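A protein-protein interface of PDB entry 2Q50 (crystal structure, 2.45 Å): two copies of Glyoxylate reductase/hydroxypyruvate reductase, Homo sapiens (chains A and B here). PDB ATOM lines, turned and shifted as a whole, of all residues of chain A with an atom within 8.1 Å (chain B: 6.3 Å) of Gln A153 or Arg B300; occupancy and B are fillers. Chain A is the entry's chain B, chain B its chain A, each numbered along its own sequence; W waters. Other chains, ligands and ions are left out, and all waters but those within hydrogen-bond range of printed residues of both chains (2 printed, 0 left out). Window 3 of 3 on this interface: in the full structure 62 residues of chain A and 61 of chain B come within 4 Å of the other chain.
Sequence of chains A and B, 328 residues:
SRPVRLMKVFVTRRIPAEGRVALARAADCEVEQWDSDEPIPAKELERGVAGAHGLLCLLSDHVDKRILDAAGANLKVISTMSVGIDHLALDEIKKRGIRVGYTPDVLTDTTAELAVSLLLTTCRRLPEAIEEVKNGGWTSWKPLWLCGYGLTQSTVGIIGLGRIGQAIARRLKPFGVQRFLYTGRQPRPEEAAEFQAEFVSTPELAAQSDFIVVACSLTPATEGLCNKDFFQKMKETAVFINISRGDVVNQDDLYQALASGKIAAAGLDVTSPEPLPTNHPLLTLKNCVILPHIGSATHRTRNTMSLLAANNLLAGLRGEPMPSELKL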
ATOM      1  N   CYS A 147      20.034  -7.807 -32.953  1.00  0.00           N
ATOM      2  CA  CYS A 147      19.435  -7.295 -31.726  1.00  0.00           C
ATOM      3  C   CYS A 147      18.666  -8.396 -31.006  1.00  0.00           C
ATOM      4  O   CYS A 147      18.053  -9.262 -31.632  1.00  0.00           O
ATOM      5  CB  CYS A 147      18.503  -6.106 -32.011  1.00  0.00           C
ATOM      6  SG  CYS A 147      19.356  -4.541 -32.406  1.00  0.00           S
ATOM      7  N   GLY A 148      18.728  -8.357 -29.680  1.00  0.00           N
ATOM      8  CA  GLY A 148      18.045  -9.339 -28.868  1.00  0.00           C
ATOM      9  C   GLY A 148      17.358  -8.612 -27.741  1.00  0.00           C
ATOM     10  O   GLY A 148      17.279  -7.384 -27.763  1.00  0.00           O
ATOM     11  N   TYR A 149      16.865  -9.365 -26.763  1.00  0.00           N
ATOM     12  CA  TYR A 149      16.176  -8.801 -25.611  1.00  0.00           C
ATOM     13  C   TYR A 149      17.070  -8.895 -24.368  1.00  0.00           C
ATOM     14  O   TYR A 149      17.655  -9.943 -24.090  1.00  0.00           O
ATOM     15  CB  TYR A 149      14.863  -9.560 -25.376  1.00  0.00           C
ATOM     16  CG  TYR A 149      13.925  -9.553 -26.575  1.00  0.00           C
ATOM     17  CD1 TYR A 149      13.051  -8.491 -26.799  1.00  0.00           C
ATOM     18  CD2 TYR A 149      13.934 -10.600 -27.498  1.00  0.00           C
ATOM     19  CE1 TYR A 149      12.208  -8.469 -27.910  1.00  0.00           C
ATOM     20  CE2 TYR A 149      13.095 -10.588 -28.614  1.00  0.00           C
ATOM     21  CZ  TYR A 149      12.236  -9.520 -28.815  1.00  0.00           C
ATOM     22  OH  TYR A 149      11.412  -9.498 -29.922  1.00  0.00           O
ATOM     23  N   GLY A 150      17.166  -7.793 -23.627  1.00  0.00           N
ATOM     24  CA  GLY A 150      17.989  -7.750 -22.429  1.00  0.00           C
ATOM     25  C   GLY A 150      17.252  -7.881 -21.105  1.00  0.00           C
ATOM     26  O   GLY A 150      16.062  -8.182 -21.069  1.00  0.00           O
ATOM     27  N   LEU A 151      17.971  -7.623 -20.015  1.00  0.00           N
ATOM     28  CA  LEU A 151      17.433  -7.740 -18.660  1.00  0.00           C
ATOM     29  C   LEU A 151      16.921  -6.462 -17.994  1.00  0.00           C
ATOM     30  O   LEU A 151      16.385  -6.522 -16.888  1.00  0.00           O
ATOM     31  CB  LEU A 151      18.486  -8.381 -17.755  1.00  0.00           C
ATOM     32  CG  LEU A 151      18.790  -9.855 -18.023  1.00  0.00           C
ATOM     33  CD1 LEU A 151      20.203 -10.174 -17.577  1.00  0.00           C
ATOM     34  CD2 LEU A 151      17.760 -10.731 -17.313  1.00  0.00           C
ATOM     35  N   THR A 152      17.083  -5.315 -18.646  1.00  0.00           N
ATOM     36  CA  THR A 152      16.616  -4.056 -18.062  1.00  0.00           C
ATOM     37  C   THR A 152      15.109  -4.074 -17.811  1.00  0.00           C
ATOM     38  O   THR A 152      14.317  -4.372 -18.706  1.00  0.00           O
ATOM     39  CB  THR A 152      16.962  -2.834 -18.961  1.00  0.00           C
ATOM     40  OG1 THR A 152      18.380  -2.607 -18.940  1.00  0.00           O
ATOM     41  CG2 THR A 152      16.268  -1.589 -18.461  1.00  0.00           C
ATOM     42  N   GLN A 153      14.720  -3.756 -16.580  1.00  0.00           N
ATOM     43  CA  GLN A 153      13.312  -3.727 -16.195  1.00  0.00           C
ATOM     44  C   GLN A 153      12.617  -5.032 -16.564  1.00  0.00           C
ATOM     45  O   GLN A 153      11.390  -5.096 -16.623  1.00  0.00           O
ATOM     46  CB  GLN A 153      12.594  -2.563 -16.887  1.00  0.00           C
ATOM     47  CG  GLN A 153      13.152  -1.184 -16.573  1.00  0.00           C
ATOM     48  CD  GLN A 153      12.379  -0.069 -17.271  1.00  0.00           C
ATOM     49  OE1 GLN A 153      12.460   0.093 -18.491  1.00  0.00           O
ATOM     50  NE2 GLN A 153      11.618   0.700 -16.497  1.00  0.00           N
ATOM     51  N   SER A 154      13.403  -6.071 -16.815  1.00  0.00           N
ATOM     52  CA  SER A 154      12.846  -7.366 -17.188  1.00  0.00           C
ATOM     53  C   SER A 154      12.258  -8.076 -15.975  1.00  0.00           C
ATOM     54  O   SER A 154      12.510  -7.693 -14.832  1.00  0.00           O
ATOM     55  CB  SER A 154      13.934  -8.258 -17.820  1.00  0.00           C
ATOM     56  OG  SER A 154      14.783  -8.832 -16.834  1.00  0.00           O
ATOM     57  N   THR A 155      11.457  -9.102 -16.232  1.00  0.00           N
ATOM     58  CA  THR A 155      10.878  -9.907 -15.163  1.00  0.00           C
ATOM     59  C   THR A 155      11.430 -11.317 -15.332  1.00  0.00           C
ATOM     60  O   THR A 155      11.178 -11.978 -16.341  1.00  0.00           O
ATOM     61  CB  THR A 155       9.355  -9.962 -15.244  1.00  0.00           C
ATOM     62  OG1 THR A 155       8.821  -8.653 -15.016  1.00  0.00           O
ATOM     63  CG2 THR A 155       8.803 -10.934 -14.200  1.00  0.00           C
ATOM     64  N   VAL A 156      12.201 -11.764 -14.349  1.00  0.00           N
ATOM     65  CA  VAL A 156      12.799 -13.080 -14.396  1.00  0.00           C
ATOM     66  C   VAL A 156      12.013 -14.105 -13.597  1.00  0.00           C
ATOM     67  O   VAL A 156      11.704 -13.892 -12.423  1.00  0.00           O
ATOM     68  CB  VAL A 156      14.255 -13.035 -13.872  1.00  0.00           C
ATOM     69  CG1 VAL A 156      14.803 -14.451 -13.699  1.00  0.00           C
ATOM     70  CG2 VAL A 156      15.124 -12.238 -14.847  1.00  0.00           C
ATOM     71  N   PHE A 175      21.619  -6.854 -12.876  1.00  0.00           N
ATOM     72  CA  PHE A 175      21.504  -6.648 -14.315  1.00  0.00           C
ATOM     73  C   PHE A 175      20.316  -5.766 -14.687  1.00  0.00           C
ATOM     74  O   PHE A 175      20.115  -5.450 -15.862  1.00  0.00           O
ATOM     75  CB  PHE A 175      21.386  -7.980 -15.049  1.00  0.00           C
ATOM     76  CG  PHE A 175      22.704  -8.569 -15.455  1.00  0.00           C
ATOM     77  CD1 PHE A 175      23.464  -9.307 -14.553  1.00  0.00           C
ATOM     78  CD2 PHE A 175      23.181  -8.394 -16.754  1.00  0.00           C
ATOM     79  CE1 PHE A 175      24.677  -9.865 -14.945  1.00  0.00           C
ATOM     80  CE2 PHE A 175      24.389  -8.947 -17.150  1.00  0.00           C
ATOM     81  CZ  PHE A 175      25.137  -9.685 -16.245  1.00  0.00           C
ATOM     82  N   GLY A 176      19.520  -5.385 -13.690  1.00  0.00           N
ATOM     83  CA  GLY A 176      18.384  -4.520 -13.957  1.00  0.00           C
ATOM     84  C   GLY A 176      17.030  -5.158 -13.748  1.00  0.00           C
ATOM     85  O   GLY A 176      15.994  -4.544 -14.018  1.00  0.00           O
ATOM     86  N   VAL A 177      17.029  -6.396 -13.273  1.00  0.00           N
ATOM     87  CA  VAL A 177      15.781  -7.097 -13.028  1.00  0.00           C
ATOM     88  C   VAL A 177      14.943  -6.307 -12.015  1.00  0.00           C
ATOM     89  O   VAL A 177      15.414  -5.974 -10.918  1.00  0.00           O
ATOM     90  CB  VAL A 177      16.047  -8.520 -12.477  1.00  0.00           C
ATOM     91  CG1 VAL A 177      14.742  -9.289 -12.348  1.00  0.00           C
ATOM     92  CG2 VAL A 177      16.998  -9.253 -13.394  1.00  0.00           C
ATOM     93  N   GLN A 178      13.708  -6.001 -12.390  1.00  0.00           N
ATOM     94  CA  GLN A 178      12.802  -5.261 -11.522  1.00  0.00           C
ATOM     95  C   GLN A 178      11.971  -6.199 -10.646  1.00  0.00           C
ATOM     96  O   GLN A 178      11.363  -5.770  -9.666  1.00  0.00           O
ATOM     97  CB  GLN A 178      11.856  -4.398 -12.366  1.00  0.00           C
ATOM     98  CG  GLN A 178      10.704  -3.799 -11.572  1.00  0.00           C
ATOM     99  CD  GLN A 178       9.701  -3.060 -12.435  1.00  0.00           C
ATOM    100  OE1 GLN A 178       8.665  -2.606 -11.945  1.00  0.00           O
ATOM    101  NE2 GLN A 178      10.001  -2.931 -13.724  1.00  0.00           N
ATOM    102  N   ARG A 179      11.958  -7.482 -10.993  1.00  0.00           N
ATOM    103  CA  ARG A 179      11.157  -8.443 -10.248  1.00  0.00           C
ATOM    104  C   ARG A 179      11.554  -9.895 -10.490  1.00  0.00           C
ATOM    105  O   ARG A 179      11.721 -10.331 -11.632  1.00  0.00           O
ATOM    106  CB  ARG A 179       9.676  -8.247 -10.613  1.00  0.00           C
ATOM    107  CG  ARG A 179       8.793  -9.454 -10.376  1.00  0.00           C
ATOM    108  CD  ARG A 179       7.378  -9.225 -10.891  1.00  0.00           C
ATOM    109  NE  ARG A 179       7.329  -8.907 -12.318  1.00  0.00           N
ATOM    110  CZ  ARG A 179       6.223  -8.958 -13.057  1.00  0.00           C
ATOM    111  NH1 ARG A 179       5.074  -9.320 -12.506  1.00  0.00           N
ATOM    112  NH2 ARG A 179       6.262  -8.637 -14.345  1.00  0.00           N
ATOM    113  N   ASP A 210       9.988 -12.559 -18.626  1.00  0.00           N
ATOM    114  CA  ASP A 210      10.720 -12.148 -19.822  1.00  0.00           C
ATOM    115  C   ASP A 210      11.854 -13.173 -19.958  1.00  0.00           C
ATOM    116  O   ASP A 210      12.425 -13.369 -21.029  1.00  0.00           O
ATOM    117  CB  ASP A 210      11.294 -10.734 -19.644  1.00  0.00           C
ATOM    118  CG  ASP A 210      10.221  -9.649 -19.697  1.00  0.00           C
ATOM    119  OD1 ASP A 210       9.609  -9.471 -20.772  1.00  0.00           O
ATOM    120  OD2 ASP A 210       9.989  -8.977 -18.668  1.00  0.00           O
ATOM    121  N   PHE A 211      12.169 -13.822 -18.842  1.00  0.00           N
ATOM    122  CA  PHE A 211      13.199 -14.853 -18.792  1.00  0.00           C
ATOM    123  C   PHE A 211      12.715 -15.934 -17.840  1.00  0.00           C
ATOM    124  O   PHE A 211      12.169 -15.637 -16.779  1.00  0.00           O
ATOM    125  CB  PHE A 211      14.541 -14.305 -18.266  1.00  0.00           C
ATOM    126  CG  PHE A 211      15.158 -13.237 -19.130  1.00  0.00           C
ATOM    127  CD1 PHE A 211      14.781 -11.906 -18.984  1.00  0.00           C
ATOM    128  CD2 PHE A 211      16.112 -13.570 -20.090  1.00  0.00           C
ATOM    129  CE1 PHE A 211      15.343 -10.917 -19.776  1.00  0.00           C
ATOM    130  CE2 PHE A 211      16.690 -12.585 -20.901  1.00  0.00           C
ATOM    131  CZ  PHE A 211      16.307 -11.255 -20.746  1.00  0.00           C
ATOM    132  N   LYS A 235       5.696 -15.456 -23.168  1.00  0.00           N
ATOM    133  CA  LYS A 235       5.729 -14.330 -24.092  1.00  0.00           C
ATOM    134  C   LYS A 235       6.574 -14.768 -25.284  1.00  0.00           C
ATOM    135  O   LYS A 235       7.660 -15.333 -25.117  1.00  0.00           O
ATOM    136  CB  LYS A 235       6.390 -13.110 -23.438  1.00  0.00           C
ATOM    137  CG  LYS A 235       5.699 -12.598 -22.193  1.00  0.00           C
ATOM    138  CD  LYS A 235       6.437 -11.404 -21.606  1.00  0.00           C
ATOM    139  CE  LYS A 235       5.798 -10.950 -20.312  1.00  0.00           C
ATOM    140  NZ  LYS A 235       6.602  -9.896 -19.639  1.00  0.00           N
ATOM    141  N   VAL B 106      22.240   6.157 -22.748  1.00  0.00           N
ATOM    142  CA  VAL B 106      21.093   5.304 -23.071  1.00  0.00           C
ATOM    143  C   VAL B 106      21.466   3.875 -23.472  1.00  0.00           C
ATOM    144  O   VAL B 106      20.597   3.006 -23.568  1.00  0.00           O
ATOM    145  CB  VAL B 106      20.238   5.909 -24.205  1.00  0.00           C
ATOM    146  CG1 VAL B 106      19.699   7.256 -23.783  1.00  0.00           C
ATOM    147  CG2 VAL B 106      21.063   6.035 -25.471  1.00  0.00           C
ATOM    148  N   THR B 298      20.267  -4.354 -28.510  1.00  0.00           N
ATOM    149  CA  THR B 298      18.971  -4.826 -28.011  1.00  0.00           C
ATOM    150  C   THR B 298      17.990  -3.872 -28.659  1.00  0.00           C
ATOM    151  O   THR B 298      18.320  -2.711 -28.918  1.00  0.00           O
ATOM    152  CB  THR B 298      18.762  -4.723 -26.472  1.00  0.00           C
ATOM    153  OG1 THR B 298      18.748  -3.344 -26.081  1.00  0.00           O
ATOM    154  CG2 THR B 298      19.827  -5.516 -25.716  1.00  0.00           C
ATOM    155  N   HIS B 299      16.788  -4.363 -28.918  1.00  0.00           N
ATOM    156  CA  HIS B 299      15.754  -3.563 -29.558  1.00  0.00           C
ATOM    157  C   HIS B 299      15.492  -2.227 -28.879  1.00  0.00           C
ATOM    158  O   HIS B 299      15.468  -1.184 -29.538  1.00  0.00           O
ATOM    159  CB  HIS B 299      14.464  -4.383 -29.647  1.00  0.00           C
ATOM    160  CG  HIS B 299      14.574  -5.557 -30.567  1.00  0.00           C
ATOM    161  ND1 HIS B 299      14.939  -5.428 -31.890  1.00  0.00           N
ATOM    162  CD2 HIS B 299      14.400  -6.883 -30.352  1.00  0.00           C
ATOM    163  CE1 HIS B 299      14.986  -6.623 -32.451  1.00  0.00           C
ATOM    164  NE2 HIS B 299      14.664  -7.524 -31.540  1.00  0.00           N
ATOM    165  N   ARG B 300      15.309  -2.261 -27.564  1.00  0.00           N
ATOM    166  CA  ARG B 300      15.035  -1.051 -26.797  1.00  0.00           C
ATOM    167  C   ARG B 300      16.183  -0.044 -26.856  1.00  0.00           C
ATOM    168  O   ARG B 300      15.957   1.157 -27.000  1.00  0.00           O
ATOM    169  CB  ARG B 300      14.720  -1.418 -25.334  1.00  0.00           C
ATOM    170  CG  ARG B 300      14.329  -0.239 -24.445  1.00  0.00           C
ATOM    171  CD  ARG B 300      13.062   0.442 -24.949  1.00  0.00           C
ATOM    172  NE  ARG B 300      11.840  -0.128 -24.383  1.00  0.00           N
ATOM    173  CZ  ARG B 300      11.414   0.082 -23.137  1.00  0.00           C
ATOM    174  NH1 ARG B 300      12.111   0.854 -22.311  1.00  0.00           N
ATOM    175  NH2 ARG B 300      10.283  -0.471 -22.718  1.00  0.00           N
ATOM    176  N   THR B 301      17.414  -0.531 -26.757  1.00  0.00           N
ATOM    177  CA  THR B 301      18.578   0.358 -26.796  1.00  0.00           C
ATOM    178  C   THR B 301      18.754   1.039 -28.141  1.00  0.00           C
ATOM    179  O   THR B 301      18.816   2.266 -28.221  1.00  0.00           O
ATOM    180  CB  THR B 301      19.873  -0.396 -26.451  1.00  0.00           C
ATOM    181  OG1 THR B 301      19.698  -1.029 -25.187  1.00  0.00           O
ATOM    182  CG2 THR B 301      21.063   0.559 -26.357  1.00  0.00           C
ATOM    183  N   ARG B 302      18.841   0.244 -29.199  1.00  0.00           N
ATOM    184  CA  ARG B 302      19.007   0.807 -30.536  1.00  0.00           C
ATOM    185  C   ARG B 302      17.874   1.769 -30.866  1.00  0.00           C
ATOM    186  O   ARG B 302      18.118   2.849 -31.403  1.00  0.00           O
ATOM    187  CB  ARG B 302      19.091  -0.307 -31.582  1.00  0.00           C
ATOM    188  CG  ARG B 302      20.384  -1.128 -31.483  1.00  0.00           C
ATOM    189  CD  ARG B 302      21.600  -0.251 -31.732  1.00  0.00           C
ATOM    190  NE  ARG B 302      22.862  -0.949 -31.498  1.00  0.00           N
ATOM    191  CZ  ARG B 302      23.308  -1.968 -32.225  1.00  0.00           C
ATOM    192  NH1 ARG B 302      22.600  -2.427 -33.253  1.00  0.00           N
ATOM    193  NH2 ARG B 302      24.463  -2.528 -31.916  1.00  0.00           N
ATOM    194  N   ASN B 303      16.640   1.396 -30.534  1.00  0.00           N
ATOM    195  CA  ASN B 303      15.505   2.276 -30.815  1.00  0.00           C
ATOM    196  C   ASN B 303      15.678   3.573 -30.036  1.00  0.00           C
ATOM    197  O   ASN B 303      15.417   4.655 -30.559  1.00  0.00           O
ATOM    198  CB  ASN B 303      14.169   1.629 -30.426  1.00  0.00           C
ATOM    199  CG  ASN B 303      13.787   0.453 -31.325  1.00  0.00           C
ATOM    200  OD1 ASN B 303      14.256   0.334 -32.463  1.00  0.00           O
ATOM    201  ND2 ASN B 303      12.909  -0.412 -30.818  1.00  0.00           N
ATOM    202  N   THR B 304      16.134   3.462 -28.790  1.00  0.00           N
ATOM    203  CA  THR B 304      16.344   4.641 -27.956  1.00  0.00           C
ATOM    204  C   THR B 304      17.464   5.498 -28.542  1.00  0.00           C
ATOM    205  O   THR B 304      17.406   6.728 -28.490  1.00  0.00           O
ATOM    206  CB  THR B 304      16.705   4.250 -26.504  1.00  0.00           C
ATOM    207  OG1 THR B 304      15.576   3.611 -25.881  1.00  0.00           O
ATOM    208  CG2 THR B 304      17.101   5.489 -25.698  1.00  0.00           C
ATOM    209  N   MET B 305      18.484   4.847 -29.098  1.00  0.00           N
ATOM    210  CA  MET B 305      19.599   5.562 -29.714  1.00  0.00           C
ATOM    211  C   MET B 305      19.104   6.318 -30.956  1.00  0.00           C
ATOM    212  O   MET B 305      19.484   7.463 -31.200  1.00  0.00           O
ATOM    213  CB  MET B 305      20.698   4.577 -30.131  1.00  0.00           C
ATOM    214  CG  MET B 305      21.429   3.915 -28.978  1.00  0.00           C
ATOM    215  SD  MET B 305      22.559   2.442 -29.530  1.00  0.00           S
ATOM    216  CE  MET B 305      24.113   3.401 -30.125  1.00  0.00           C
HETATM  217  O   HOH W   1      12.532  -1.805 -20.552  1.00  0.00           O
HETATM  218  O   HOH W   2      15.586 -10.512 -30.529  1.00  0.00           O
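The backbone NH of His B299 is in hydrogen-bond range of the backbone carbonyl oxygen of Gly A148, at 3.3 Å.
OG1 of Thr B301 sits at hydrogen-bond distance from OG1 of Thr B298, 2.7 Å away.
The backbone carbonyl oxygen (O) of His B299 sits close to the side-chain amide nitrogen (ND2) of Asn B303.
The side-chain hydroxyl of Thr B304 sits at hydrogen-bond distance from the backbone carbonyl oxygen of Arg B300 (2.7 Å).
The backbone carbonyl oxygen of Gly A176 is in hydrogen-bond range of the backbone NH of Gln A153, 3.0 Å away.
CB of Cys A147 touches CE1 of His B299 (3.6 Å).
CG of Arg B302 touches SG of Cys A147, 3.7 Å away.
Gly A148 touches Thr B298 (O to CA, 3.1 Å).
His B299 touches Tyr A149.
Arg B300 touches Gln A153.
Of the printed residues of chain B, Cys A147 touches His B299 and Arg B302.
Of the printed residues of chain B, Tyr A149 touches His B299 (3.6 Å).
Gln A153 touches just one residue of chain B: Arg B300.
Val A156 touches none of the printed residues of chain B.
Printed residues of chain A within 4 Å of Thr B298: Gly A148 (3.1 Å).
Arg B300 touches just one residue of chain A: Gln A153.
The nearest printed residue of chain B that does not touch Gln A153 is Thr B304 (8.8 Å).
The nearest residue of chain A that does not touch Arg B300 is Gly A148 (5.5 Å).
The nearest printed residue of chain A that does not touch Arg B302 is Gly A148 (7.6 Å).
Of the 9 printed residues of chain B, 4 touch a printed residue of chain A.
Printed residues of chain B that touch a printed residue of chain A: Thr B298, His B299, Arg B300 and Arg B302.
Hydrophobic or aromatic side chains of chain B within 4 Å of the printed part of chain A: His B299.
Hydrophobic or aromatic side chains of chain A within 4 Å of the printed part of chain B: Tyr A149.
Among the printed residues, 6 pairs touch across the chains.
No position is printed for both chains.
Of the 6 pairs that touch across the chains among the printed residues, none has its exchanged pair printed and touching as well.
Water W1 lies within hydrogen-bond range of OE1 of Gln A153 (2.8 Å) and NH1 of Arg B300 (3.2 Å).
Water W2 lies within hydrogen-bond range of O of Cys A147 (3.0 Å) and NE2 of His B299 (3.3 Å).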
